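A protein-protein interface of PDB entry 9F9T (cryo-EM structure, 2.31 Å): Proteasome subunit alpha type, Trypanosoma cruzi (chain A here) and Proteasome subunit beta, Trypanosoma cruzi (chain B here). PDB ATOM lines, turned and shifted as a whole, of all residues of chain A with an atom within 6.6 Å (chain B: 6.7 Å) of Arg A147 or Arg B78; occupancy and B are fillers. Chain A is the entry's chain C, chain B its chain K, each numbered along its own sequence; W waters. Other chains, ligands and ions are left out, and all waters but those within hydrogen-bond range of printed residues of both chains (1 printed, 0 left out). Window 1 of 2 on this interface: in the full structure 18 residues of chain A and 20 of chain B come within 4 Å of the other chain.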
ATOM      1  N   GLN A 108     -14.697 -25.490 -18.958  1.00  0.00           N
ATOM      2  CA  GLN A 108     -13.740 -24.403 -18.776  1.00  0.00           C
ATOM      3  C   GLN A 108     -14.198 -23.371 -17.751  1.00  0.00           C
ATOM      4  O   GLN A 108     -13.999 -22.186 -17.945  1.00  0.00           O
ATOM      5  CB  GLN A 108     -13.462 -23.646 -20.079  1.00  0.00           C
ATOM      6  CG  GLN A 108     -12.845 -24.518 -21.154  1.00  0.00           C
ATOM      7  CD  GLN A 108     -11.470 -25.053 -20.818  1.00  0.00           C
ATOM      8  OE1 GLN A 108     -10.606 -24.319 -20.330  1.00  0.00           O
ATOM      9  NE2 GLN A 108     -11.266 -26.343 -21.063  1.00  0.00           N
ATOM     10  N   GLU A 109     -14.696 -23.839 -16.621  1.00  0.00           N
ATOM     11  CA  GLU A 109     -15.111 -22.968 -15.543  1.00  0.00           C
ATOM     12  C   GLU A 109     -14.896 -23.763 -14.248  1.00  0.00           C
ATOM     13  O   GLU A 109     -14.868 -24.973 -14.243  1.00  0.00           O
ATOM     14  CB  GLU A 109     -16.569 -22.508 -15.748  1.00  0.00           C
ATOM     15  CG  GLU A 109     -17.561 -23.497 -15.106  1.00  0.00           C
ATOM     16  CD  GLU A 109     -19.078 -23.267 -15.095  1.00  0.00           C
ATOM     17  OE1 GLU A 109     -19.818 -24.318 -14.992  1.00  0.00           O
ATOM     18  OE2 GLU A 109     -19.545 -22.067 -15.159  1.00  0.00           O
ATOM     19  N   TRP A 145     -15.111 -21.360  -2.673  1.00  0.00           N
ATOM     20  CA  TRP A 145     -15.708 -20.139  -3.153  1.00  0.00           C
ATOM     21  C   TRP A 145     -16.218 -20.387  -4.546  1.00  0.00           C
ATOM     22  O   TRP A 145     -15.490 -20.974  -5.314  1.00  0.00           O
ATOM     23  CB  TRP A 145     -14.734 -18.963  -3.152  1.00  0.00           C
ATOM     24  CG  TRP A 145     -15.493 -17.708  -3.448  1.00  0.00           C
ATOM     25  CD1 TRP A 145     -16.127 -16.859  -2.589  1.00  0.00           C
ATOM     26  CD2 TRP A 145     -15.778 -17.218  -4.778  1.00  0.00           C
ATOM     27  NE1 TRP A 145     -16.757 -15.859  -3.290  1.00  0.00           N
ATOM     28  CE2 TRP A 145     -16.549 -16.042  -4.625  1.00  0.00           C
ATOM     29  CE3 TRP A 145     -15.419 -17.648  -6.064  1.00  0.00           C
ATOM     30  CZ2 TRP A 145     -16.984 -15.307  -5.720  1.00  0.00           C
ATOM     31  CZ3 TRP A 145     -15.834 -16.904  -7.142  1.00  0.00           C
ATOM     32  CH2 TRP A 145     -16.624 -15.764  -6.970  1.00  0.00           C
ATOM     33  N   ASP A 146     -17.495 -20.065  -4.802  1.00  0.00           N
ATOM     34  CA  ASP A 146     -18.035 -19.980  -6.143  1.00  0.00           C
ATOM     35  C   ASP A 146     -18.985 -18.807  -6.254  1.00  0.00           C
ATOM     36  O   ASP A 146     -19.432 -18.239  -5.257  1.00  0.00           O
ATOM     37  CB  ASP A 146     -18.755 -21.244  -6.573  1.00  0.00           C
ATOM     38  CG  ASP A 146     -19.883 -21.642  -5.647  1.00  0.00           C
ATOM     39  OD1 ASP A 146     -20.708 -20.751  -5.344  1.00  0.00           O
ATOM     40  OD2 ASP A 146     -19.961 -22.859  -5.261  1.00  0.00           O
ATOM     41  N   ARG A 147     -19.317 -18.463  -7.499  1.00  0.00           N
ATOM     42  CA  ARG A 147     -20.109 -17.277  -7.772  1.00  0.00           C
ATOM     43  C   ARG A 147     -21.595 -17.531  -7.479  1.00  0.00           C
ATOM     44  O   ARG A 147     -22.390 -16.607  -7.402  1.00  0.00           O
ATOM     45  CB  ARG A 147     -19.857 -16.846  -9.220  1.00  0.00           C
ATOM     46  CG  ARG A 147     -20.311 -17.848 -10.280  1.00  0.00           C
ATOM     47  CD  ARG A 147     -20.296 -17.263 -11.690  1.00  0.00           C
ATOM     48  NE  ARG A 147     -20.872 -18.198 -12.652  1.00  0.00           N
ATOM     49  CZ  ARG A 147     -21.934 -17.957 -13.425  1.00  0.00           C
ATOM     50  NH1 ARG A 147     -22.464 -18.936 -14.142  1.00  0.00           N
ATOM     51  NH2 ARG A 147     -22.490 -16.754 -13.447  1.00  0.00           N
ATOM     52  N   HIS A 148     -21.991 -18.790  -7.339  1.00  0.00           N
ATOM     53  CA  HIS A 148     -23.381 -19.084  -7.058  1.00  0.00           C
ATOM     54  C   HIS A 148     -23.678 -18.704  -5.608  1.00  0.00           C
ATOM     55  O   HIS A 148     -24.672 -18.036  -5.358  1.00  0.00           O
ATOM     56  CB  HIS A 148     -23.717 -20.526  -7.457  1.00  0.00           C
ATOM     57  CG  HIS A 148     -23.503 -20.840  -8.915  1.00  0.00           C
ATOM     58  ND1 HIS A 148     -23.455 -19.881  -9.908  1.00  0.00           N
ATOM     59  CD2 HIS A 148     -23.340 -22.025  -9.543  1.00  0.00           C
ATOM     60  CE1 HIS A 148     -23.246 -20.474 -11.081  1.00  0.00           C
ATOM     61  NE2 HIS A 148     -23.174 -21.772 -10.884  1.00  0.00           N
ATOM     62  N   HIS A 149     -22.750 -19.033  -4.687  1.00  0.00           N
ATOM     63  CA  HIS A 149     -23.052 -19.077  -3.262  1.00  0.00           C
ATOM     64  C   HIS A 149     -22.025 -18.394  -2.351  1.00  0.00           C
ATOM     65  O   HIS A 149     -22.174 -18.471  -1.140  1.00  0.00           O
ATOM     66  CB  HIS A 149     -23.202 -20.533  -2.823  1.00  0.00           C
ATOM     67  CG  HIS A 149     -24.388 -21.243  -3.371  1.00  0.00           C
ATOM     68  ND1 HIS A 149     -25.669 -20.731  -3.280  1.00  0.00           N
ATOM     69  CD2 HIS A 149     -24.485 -22.445  -3.998  1.00  0.00           C
ATOM     70  CE1 HIS A 149     -26.505 -21.586  -3.869  1.00  0.00           C
ATOM     71  NE2 HIS A 149     -25.812 -22.642  -4.307  1.00  0.00           N
ATOM     72  N   GLY A 150     -21.005 -17.726  -2.896  1.00  0.00           N
ATOM     73  CA  GLY A 150     -19.932 -17.166  -2.072  1.00  0.00           C
ATOM     74  C   GLY A 150     -19.133 -18.203  -1.271  1.00  0.00           C
ATOM     75  O   GLY A 150     -19.047 -19.373  -1.652  1.00  0.00           O
ATOM     76  N   GLN A 152     -18.241 -20.887   1.435  1.00  0.00           N
ATOM     77  CA  GLN A 152     -19.008 -22.036   1.814  1.00  0.00           C
ATOM     78  C   GLN A 152     -18.064 -22.941   2.542  1.00  0.00           C
ATOM     79  O   GLN A 152     -16.941 -23.061   2.087  1.00  0.00           O
ATOM     80  CB  GLN A 152     -19.476 -22.777   0.589  1.00  0.00           C
ATOM     81  CG  GLN A 152     -20.530 -21.990  -0.167  1.00  0.00           C
ATOM     82  CD  GLN A 152     -20.679 -22.532  -1.560  1.00  0.00           C
ATOM     83  OE1 GLN A 152     -21.439 -23.447  -1.812  1.00  0.00           O
ATOM     84  NE2 GLN A 152     -19.922 -21.947  -2.470  1.00  0.00           N
ATOM     85  N   VAL A 238     -11.674 -12.524 -19.951  1.00  0.00           N
ATOM     86  CA  VAL A 238     -12.147 -11.567 -18.967  1.00  0.00           C
ATOM     87  C   VAL A 238     -11.922 -12.182 -17.588  1.00  0.00           C
ATOM     88  O   VAL A 238     -12.405 -13.281 -17.307  1.00  0.00           O
ATOM     89  CB  VAL A 238     -13.620 -11.151 -19.195  1.00  0.00           C
ATOM     90  CG1 VAL A 238     -13.989  -9.903 -18.392  1.00  0.00           C
ATOM     91  CG2 VAL A 238     -13.933 -10.937 -20.673  1.00  0.00           C
ATOM     92  N   ASP B  40     -32.000 -22.215 -23.266  1.00  0.00           N
ATOM     93  CA  ASP B  40     -32.306 -21.825 -21.912  1.00  0.00           C
ATOM     94  C   ASP B  40     -32.910 -20.445 -21.975  1.00  0.00           C
ATOM     95  O   ASP B  40     -33.381 -20.026 -23.010  1.00  0.00           O
ATOM     96  CB  ASP B  40     -31.137 -22.058 -20.981  1.00  0.00           C
ATOM     97  CG  ASP B  40     -30.149 -20.937 -20.635  1.00  0.00           C
ATOM     98  OD1 ASP B  40     -30.404 -19.730 -20.900  1.00  0.00           O
ATOM     99  OD2 ASP B  40     -29.100 -21.300 -20.008  1.00  0.00           O
ATOM    100  N   LYS B  43     -30.318 -18.150 -23.848  1.00  0.00           N
ATOM    101  CA  LYS B  43     -29.487 -18.713 -24.889  1.00  0.00           C
ATOM    102  C   LYS B  43     -30.262 -19.187 -26.101  1.00  0.00           C
ATOM    103  O   LYS B  43     -31.364 -19.677 -25.949  1.00  0.00           O
ATOM    104  CB  LYS B  43     -28.669 -19.871 -24.345  1.00  0.00           C
ATOM    105  CG  LYS B  43     -27.564 -19.423 -23.429  1.00  0.00           C
ATOM    106  CD  LYS B  43     -26.907 -20.619 -22.788  1.00  0.00           C
ATOM    107  CE  LYS B  43     -26.015 -20.212 -21.635  1.00  0.00           C
ATOM    108  NZ  LYS B  43     -26.745 -19.456 -20.577  1.00  0.00           N
ATOM    109  N   MET B  65     -27.821 -29.743 -20.369  1.00  0.00           N
ATOM    110  CA  MET B  65     -27.824 -28.495 -19.652  1.00  0.00           C
ATOM    111  C   MET B  65     -28.915 -28.520 -18.599  1.00  0.00           C
ATOM    112  O   MET B  65     -28.794 -27.885 -17.574  1.00  0.00           O
ATOM    113  CB  MET B  65     -28.113 -27.295 -20.575  1.00  0.00           C
ATOM    114  CG  MET B  65     -26.889 -26.932 -21.414  1.00  0.00           C
ATOM    115  SD  MET B  65     -27.236 -25.591 -22.519  1.00  0.00           S
ATOM    116  CE  MET B  65     -27.341 -24.291 -21.277  1.00  0.00           C
ATOM    117  N   LYS B  68     -27.764 -30.224 -15.698  1.00  0.00           N
ATOM    118  CA  LYS B  68     -26.782 -29.469 -14.928  1.00  0.00           C
ATOM    119  C   LYS B  68     -27.487 -28.415 -14.077  1.00  0.00           C
ATOM    120  O   LYS B  68     -26.926 -27.888 -13.135  1.00  0.00           O
ATOM    121  CB  LYS B  68     -25.776 -28.757 -15.826  1.00  0.00           C
ATOM    122  CG  LYS B  68     -24.349 -28.763 -15.313  1.00  0.00           C
ATOM    123  CD  LYS B  68     -23.435 -27.706 -15.968  1.00  0.00           C
ATOM    124  CE  LYS B  68     -22.368 -27.176 -15.023  1.00  0.00           C
ATOM    125  NZ  LYS B  68     -21.889 -25.829 -15.436  1.00  0.00           N
ATOM    126  N   ARG B  75     -29.289 -22.891 -11.189  1.00  0.00           N
ATOM    127  CA  ARG B  75     -28.340 -21.839 -11.475  1.00  0.00           C
ATOM    128  C   ARG B  75     -28.018 -21.869 -12.965  1.00  0.00           C
ATOM    129  O   ARG B  75     -27.669 -22.915 -13.498  1.00  0.00           O
ATOM    130  CB  ARG B  75     -27.109 -21.979 -10.574  1.00  0.00           C
ATOM    131  CG  ARG B  75     -26.842 -20.730  -9.739  1.00  0.00           C
ATOM    132  CD  ARG B  75     -28.066 -20.245  -8.962  1.00  0.00           C
ATOM    133  NE  ARG B  75     -27.792 -19.157  -8.025  1.00  0.00           N
ATOM    134  CZ  ARG B  75     -28.107 -19.163  -6.731  1.00  0.00           C
ATOM    135  NH1 ARG B  75     -28.701 -20.214  -6.190  1.00  0.00           N
ATOM    136  NH2 ARG B  75     -27.821 -18.112  -5.982  1.00  0.00           N
ATOM    137  N   VAL B  76     -28.130 -20.698 -13.610  1.00  0.00           N
ATOM    138  CA  VAL B  76     -27.885 -20.549 -15.037  1.00  0.00           C
ATOM    139  C   VAL B  76     -26.383 -20.656 -15.326  1.00  0.00           C
ATOM    140  O   VAL B  76     -25.501 -20.070 -14.706  1.00  0.00           O
ATOM    141  CB  VAL B  76     -28.493 -19.240 -15.585  1.00  0.00           C
ATOM    142  CG1 VAL B  76     -28.428 -19.159 -17.104  1.00  0.00           C
ATOM    143  CG2 VAL B  76     -29.937 -19.049 -15.137  1.00  0.00           C
ATOM    144  N   ILE B  77     -26.095 -21.430 -16.344  1.00  0.00           N
ATOM    145  CA  ILE B  77     -24.742 -21.627 -16.786  1.00  0.00           C
ATOM    146  C   ILE B  77     -24.330 -20.496 -17.713  1.00  0.00           C
ATOM    147  O   ILE B  77     -25.139 -19.933 -18.451  1.00  0.00           O
ATOM    148  CB  ILE B  77     -24.685 -23.018 -17.410  1.00  0.00           C
ATOM    149  CG1 ILE B  77     -23.553 -23.195 -18.409  1.00  0.00           C
ATOM    150  CG2 ILE B  77     -26.028 -23.390 -17.986  1.00  0.00           C
ATOM    151  CD1 ILE B  77     -23.453 -24.621 -18.965  1.00  0.00           C
ATOM    152  N   ARG B  78     -23.058 -20.132 -17.628  1.00  0.00           N
ATOM    153  CA  ARG B  78     -22.541 -19.062 -18.472  1.00  0.00           C
ATOM    154  C   ARG B  78     -22.484 -19.492 -19.915  1.00  0.00           C
ATOM    155  O   ARG B  78     -22.090 -20.626 -20.208  1.00  0.00           O
ATOM    156  CB  ARG B  78     -21.049 -18.822 -18.261  1.00  0.00           C
ATOM    157  CG  ARG B  78     -20.648 -18.065 -17.028  1.00  0.00           C
ATOM    158  CD  ARG B  78     -19.149 -18.345 -16.936  1.00  0.00           C
ATOM    159  NE  ARG B  78     -18.443 -17.375 -17.755  1.00  0.00           N
ATOM    160  CZ  ARG B  78     -17.923 -16.254 -17.283  1.00  0.00           C
ATOM    161  NH1 ARG B  78     -17.776 -15.220 -18.096  1.00  0.00           N
ATOM    162  NH2 ARG B  78     -17.691 -16.139 -15.985  1.00  0.00           N
ATOM    163  N   THR B  79     -22.591 -18.490 -20.768  1.00  0.00           N
ATOM    164  CA  THR B  79     -22.502 -18.750 -22.199  1.00  0.00           C
ATOM    165  C   THR B  79     -21.189 -19.402 -22.576  1.00  0.00           C
ATOM    166  O   THR B  79     -21.160 -20.326 -23.390  1.00  0.00           O
ATOM    167  CB  THR B  79     -22.659 -17.486 -23.008  1.00  0.00           C
ATOM    168  OG1 THR B  79     -23.875 -16.868 -22.598  1.00  0.00           O
ATOM    169  CG2 THR B  79     -22.784 -17.793 -24.466  1.00  0.00           C
ATOM    170  N   SER B  80     -20.093 -19.002 -21.926  1.00  0.00           N
ATOM    171  CA  SER B  80     -18.815 -19.567 -22.338  1.00  0.00           C
ATOM    172  C   SER B  80     -18.659 -21.022 -21.903  1.00  0.00           C
ATOM    173  O   SER B  80     -17.884 -21.749 -22.477  1.00  0.00           O
ATOM    174  CB  SER B  80     -17.683 -18.758 -21.869  1.00  0.00           C
ATOM    175  OG  SER B  80     -17.360 -19.147 -20.553  1.00  0.00           O
ATOM    176  N   ALA B  81     -19.437 -21.461 -20.925  1.00  0.00           N
ATOM    177  CA  ALA B  81     -19.421 -22.854 -20.528  1.00  0.00           C
ATOM    178  C   ALA B  81     -20.301 -23.688 -21.423  1.00  0.00           C
ATOM    179  O   ALA B  81     -20.003 -24.850 -21.642  1.00  0.00           O
ATOM    180  CB  ALA B  81     -19.869 -23.030 -19.109  1.00  0.00           C
ATOM    181  N   ALA B  82     -21.417 -23.140 -21.864  1.00  0.00           N
ATOM    182  CA  ALA B  82     -22.282 -23.857 -22.788  1.00  0.00           C
ATOM    183  C   ALA B  82     -21.522 -24.072 -24.078  1.00  0.00           C
ATOM    184  O   ALA B  82     -21.488 -25.185 -24.562  1.00  0.00           O
ATOM    185  CB  ALA B  82     -23.593 -23.167 -22.947  1.00  0.00           C
ATOM    186  N   ALA B  83     -20.732 -23.100 -24.481  1.00  0.00           N
ATOM    187  CA  ALA B  83     -19.961 -23.216 -25.727  1.00  0.00           C
ATOM    188  C   ALA B  83     -18.848 -24.234 -25.578  1.00  0.00           C
ATOM    189  O   ALA B  83     -18.604 -25.053 -26.450  1.00  0.00           O
ATOM    190  CB  ALA B  83     -19.398 -21.889 -26.055  1.00  0.00           C
ATOM    191  N   LEU B 107     -23.694 -19.969 -31.338  1.00  0.00           N
ATOM    192  CA  LEU B 107     -24.284 -19.904 -30.050  1.00  0.00           C
ATOM    193  C   LEU B 107     -24.280 -18.493 -29.523  1.00  0.00           C
ATOM    194  O   LEU B 107     -23.237 -17.865 -29.467  1.00  0.00           O
ATOM    195  CB  LEU B 107     -23.481 -20.807 -29.155  1.00  0.00           C
ATOM    196  CG  LEU B 107     -23.913 -20.694 -27.687  1.00  0.00           C
ATOM    197  CD1 LEU B 107     -25.235 -21.364 -27.496  1.00  0.00           C
ATOM    198  CD2 LEU B 107     -22.924 -21.332 -26.739  1.00  0.00           C
ATOM    199  N   ASP B 111     -25.242 -13.091 -20.534  1.00  0.00           N
ATOM    200  CA  ASP B 111     -24.898 -13.604 -19.205  1.00  0.00           C
ATOM    201  C   ASP B 111     -25.360 -12.607 -18.161  1.00  0.00           C
ATOM    202  O   ASP B 111     -25.187 -11.407 -18.291  1.00  0.00           O
ATOM    203  CB  ASP B 111     -23.416 -13.890 -19.030  1.00  0.00           C
ATOM    204  CG  ASP B 111     -22.926 -15.124 -19.772  1.00  0.00           C
ATOM    205  OD1 ASP B 111     -23.700 -15.672 -20.501  1.00  0.00           O
ATOM    206  OD2 ASP B 111     -21.751 -15.506 -19.637  1.00  0.00           O
ATOM    207  N   VAL B 112     -25.949 -13.144 -17.103  1.00  0.00           N
ATOM    208  CA  VAL B 112     -26.631 -12.312 -16.124  1.00  0.00           C
ATOM    209  C   VAL B 112     -26.266 -12.834 -14.730  1.00  0.00           C
ATOM    210  O   VAL B 112     -26.221 -14.050 -14.548  1.00  0.00           O
ATOM    211  CB  VAL B 112     -28.135 -12.353 -16.469  1.00  0.00           C
ATOM    212  CG1 VAL B 112     -28.858 -13.479 -15.724  1.00  0.00           C
ATOM    213  CG2 VAL B 112     -28.789 -10.999 -16.263  1.00  0.00           C
ATOM    214  N   ALA B 113     -25.966 -11.937 -13.770  1.00  0.00           N
ATOM    215  CA  ALA B 113     -25.417 -12.328 -12.460  1.00  0.00           C
ATOM    216  C   ALA B 113     -26.313 -13.327 -11.710  1.00  0.00           C
ATOM    217  O   ALA B 113     -27.494 -13.064 -11.469  1.00  0.00           O
ATOM    218  CB  ALA B 113     -25.161 -11.098 -11.622  1.00  0.00           C
ATOM    219  N   ALA B 114     -25.739 -14.491 -11.361  1.00  0.00           N
ATOM    220  CA  ALA B 114     -26.409 -15.516 -10.562  1.00  0.00           C
ATOM    221  C   ALA B 114     -26.912 -14.931  -9.239  1.00  0.00           C
ATOM    222  O   ALA B 114     -28.122 -14.887  -9.001  1.00  0.00           O
ATOM    223  CB  ALA B 114     -25.476 -16.690 -10.309  1.00  0.00           C
ATOM    224  N   SER B 115     -25.965 -14.478  -8.399  1.00  0.00           N
ATOM    225  CA  SER B 115     -26.254 -13.936  -7.079  1.00  0.00           C
ATOM    226  C   SER B 115     -25.595 -12.562  -6.930  1.00  0.00           C
ATOM    227  O   SER B 115     -25.248 -11.933  -7.933  1.00  0.00           O
ATOM    228  CB  SER B 115     -25.831 -14.929  -6.003  1.00  0.00           C
ATOM    229  OG  SER B 115     -24.473 -15.329  -6.142  1.00  0.00           O
ATOM    230  N   SER B 116     -25.450 -12.091  -5.680  1.00  0.00           N
ATOM    231  CA  SER B 116     -24.748 -10.847  -5.380  1.00  0.00           C
ATOM    232  C   SER B 116     -23.236 -11.078  -5.276  1.00  0.00           C
ATOM    233  O   SER B 116     -22.457 -10.193  -5.641  1.00  0.00           O
ATOM    234  CB  SER B 116     -25.322 -10.199  -4.132  1.00  0.00           C
ATOM    235  OG  SER B 116     -25.895 -11.170  -3.267  1.00  0.00           O
ATOM    236  N   ASP B 117     -22.847 -12.280  -4.802  1.00  0.00           N
ATOM    237  CA  ASP B 117     -21.458 -12.731  -4.703  1.00  0.00           C
ATOM    238  C   ASP B 117     -20.783 -12.741  -6.082  1.00  0.00           C
ATOM    239  O   ASP B 117     -19.568 -12.568  -6.185  1.00  0.00           O
ATOM    240  CB  ASP B 117     -21.357 -14.142  -4.098  1.00  0.00           C
ATOM    241  CG  ASP B 117     -22.168 -14.407  -2.829  1.00  0.00           C
ATOM    242  OD1 ASP B 117     -21.847 -13.804  -1.779  1.00  0.00           O
ATOM    243  OD2 ASP B 117     -23.105 -15.248  -2.889  1.00  0.00           O
ATOM    244  N   ASP B 118     -21.605 -12.909  -7.127  1.00  0.00           N
ATOM    245  CA  ASP B 118     -21.197 -13.077  -8.513  1.00  0.00           C
ATOM    246  C   ASP B 118     -20.621 -11.787  -9.125  1.00  0.00           C
ATOM    247  O   ASP B 118     -21.307 -10.778  -9.245  1.00  0.00           O
ATOM    248  CB  ASP B 118     -22.395 -13.617  -9.306  1.00  0.00           C
ATOM    249  CG  ASP B 118     -22.074 -14.249 -10.654  1.00  0.00           C
ATOM    250  OD1 ASP B 118     -20.870 -14.298 -11.021  1.00  0.00           O
ATOM    251  OD2 ASP B 118     -23.029 -14.703 -11.330  1.00  0.00           O
ATOM    252  N   ASP B 119     -19.381 -11.905  -9.617  1.00  0.00           N
ATOM    253  CA  ASP B 119     -18.540 -10.825 -10.113  1.00  0.00           C
ATOM    254  C   ASP B 119     -18.549 -10.770 -11.648  1.00  0.00           C
ATOM    255  O   ASP B 119     -17.907  -9.897 -12.248  1.00  0.00           O
ATOM    256  CB  ASP B 119     -17.105 -11.009  -9.588  1.00  0.00           C
ATOM    257  CG  ASP B 119     -16.611 -12.458  -9.474  1.00  0.00           C
ATOM    258  OD1 ASP B 119     -17.211 -13.366 -10.104  1.00  0.00           O
ATOM    259  OD2 ASP B 119     -15.635 -12.689  -8.724  1.00  0.00           O
ATOM    260  N   ILE B 120     -19.299 -11.701 -12.268  1.00  0.00           N
ATOM    261  CA  ILE B 120     -19.299 -11.951 -13.706  1.00  0.00           C
ATOM    262  C   ILE B 120     -19.550 -10.650 -14.468  1.00  0.00           C
ATOM    263  O   ILE B 120     -20.460  -9.891 -14.133  1.00  0.00           O
ATOM    264  CB  ILE B 120     -20.347 -13.035 -14.076  1.00  0.00           C
ATOM    265  CG1 ILE B 120     -20.242 -13.492 -15.538  1.00  0.00           C
ATOM    266  CG2 ILE B 120     -21.763 -12.571 -13.756  1.00  0.00           C
ATOM    267  CD1 ILE B 120     -21.218 -14.587 -15.946  1.00  0.00           C
ATOM    268  N   ALA B 121     -18.743 -10.414 -15.510  1.00  0.00           N
ATOM    269  CA  ALA B 121     -19.103  -9.441 -16.528  1.00  0.00           C
ATOM    270  C   ALA B 121     -20.399  -9.893 -17.201  1.00  0.00           C
ATOM    271  O   ALA B 121     -20.480 -10.971 -17.797  1.00  0.00           O
ATOM    272  CB  ALA B 121     -17.988  -9.244 -17.528  1.00  0.00           C
ATOM    273  N   HIS B 125     -22.731 -12.545 -25.585  1.00  0.00           N
ATOM    274  CA  HIS B 125     -21.610 -13.178 -26.194  1.00  0.00           C
ATOM    275  C   HIS B 125     -22.049 -14.043 -27.342  1.00  0.00           C
ATOM    276  O   HIS B 125     -22.919 -14.871 -27.161  1.00  0.00           O
ATOM    277  CB  HIS B 125     -20.989 -14.098 -25.177  1.00  0.00           C
ATOM    278  CG  HIS B 125     -20.437 -13.271 -24.057  1.00  0.00           C
ATOM    279  ND1 HIS B 125     -19.202 -12.647 -24.166  1.00  0.00           N
ATOM    280  CD2 HIS B 125     -20.893 -13.024 -22.791  1.00  0.00           C
ATOM    281  CE1 HIS B 125     -18.947 -12.057 -23.002  1.00  0.00           C
ATOM    282  NE2 HIS B 125     -19.977 -12.234 -22.178  1.00  0.00           N
HETATM  283  O   HOH W   1     -16.126 -21.542 -19.635  1.00  0.00           O
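NZ of Lys B68 lies within salt-bridge range of OE1 of Glu A109 (2.6 Å).
The guanidinium group of Arg B75 sits at hydrogen-bond distance from the backbone carbonyl oxygen of His A148 (3.2 Å).
NH1 of Arg A147 lies within hydrogen-bond range of O of Val B76 (3.3 Å).
The side-chain hydroxyl of Ser B115 lies within hydrogen-bond range of the backbone carbonyl oxygen of Arg A147, 2.7 Å away.
OG of Ser B115 sits at hydrogen-bond distance from O of His A148 (2.8 Å).
OD2 of Asp B117 is in hydrogen-bond range of N of Gly A150.
The side-chain carboxylate of Asp B118 lies within salt-bridge range of the guanidinium group of Arg A147.
NE of Arg B78 is in hydrogen-bond range of OG of Ser B80, at 3.5 Å.
The side-chain carboxylate (OD2) of Asp B118 is in hydrogen-bond range of the backbone NH (N) of Ala B114 (2.7 Å).
The side-chain carboxylate of Asp B118 sits at hydrogen-bond distance from the backbone NH of Ile B120 (3.3 Å).
The backbone NH (N) of His A148 sits at hydrogen-bond distance from the side-chain carboxylate (OD1) of Asp A146, 3.1 Å away.
OD1 of Asp A146 sits at hydrogen-bond distance from N of His A149 (2.7 Å).
The backbone carbonyl oxygen (O) of Gly A150 lies within hydrogen-bond range of the side-chain amide nitrogen (NE2) of Gln A152 (2.8 Å).
Among the printed residues, pairs that only touch across the chains: Trp A145 with Asp B117 (3.8 Å), Trp A145 with Asp B119 (3.7 Å), Arg A147 with Arg B78 (3.5 Å), Arg A147 with Ile B120 (3.5 Å), His A148 with Ala B114 (3.8 Å), His A149 with Arg B75 (3.5 Å) and His A149 with Asp B117 (3.4 Å).
Of chain B, only Val B76, Arg B78, Ser B115, Asp B118 and Ile B120 come within 4 Å of Arg A147.
Lys B43 touches none of the printed residues of chain A.
Of chain A, only Arg A147 (3.5 Å) comes within 4 Å of Arg B78.
Of the printed residues of chain A, Ala B114 touches His A148 (3.8 Å).
Ser B116 touches none of the printed residues of chain A.
Of the printed residues of chain A, Asp B118 touches Arg A147 (3.0 Å).
Of the printed residues of chain A, Asp B119 touches Trp A145.
Of the 10 printed residues of chain A, 6 touch a printed residue of chain B.
Hydrophobic or aromatic side chains of chain A that line the printed part of chain B: Trp A145, His A148 and His A149.
Along chain A the printed residues that touch a printed residue of chain B span positions 109 to 150.
Water W1 bridges the backbone carbonyl oxygen of Gln A108 (2.8 Å) and the side-chain hydroxyl of Ser B80 (2.8 Å).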
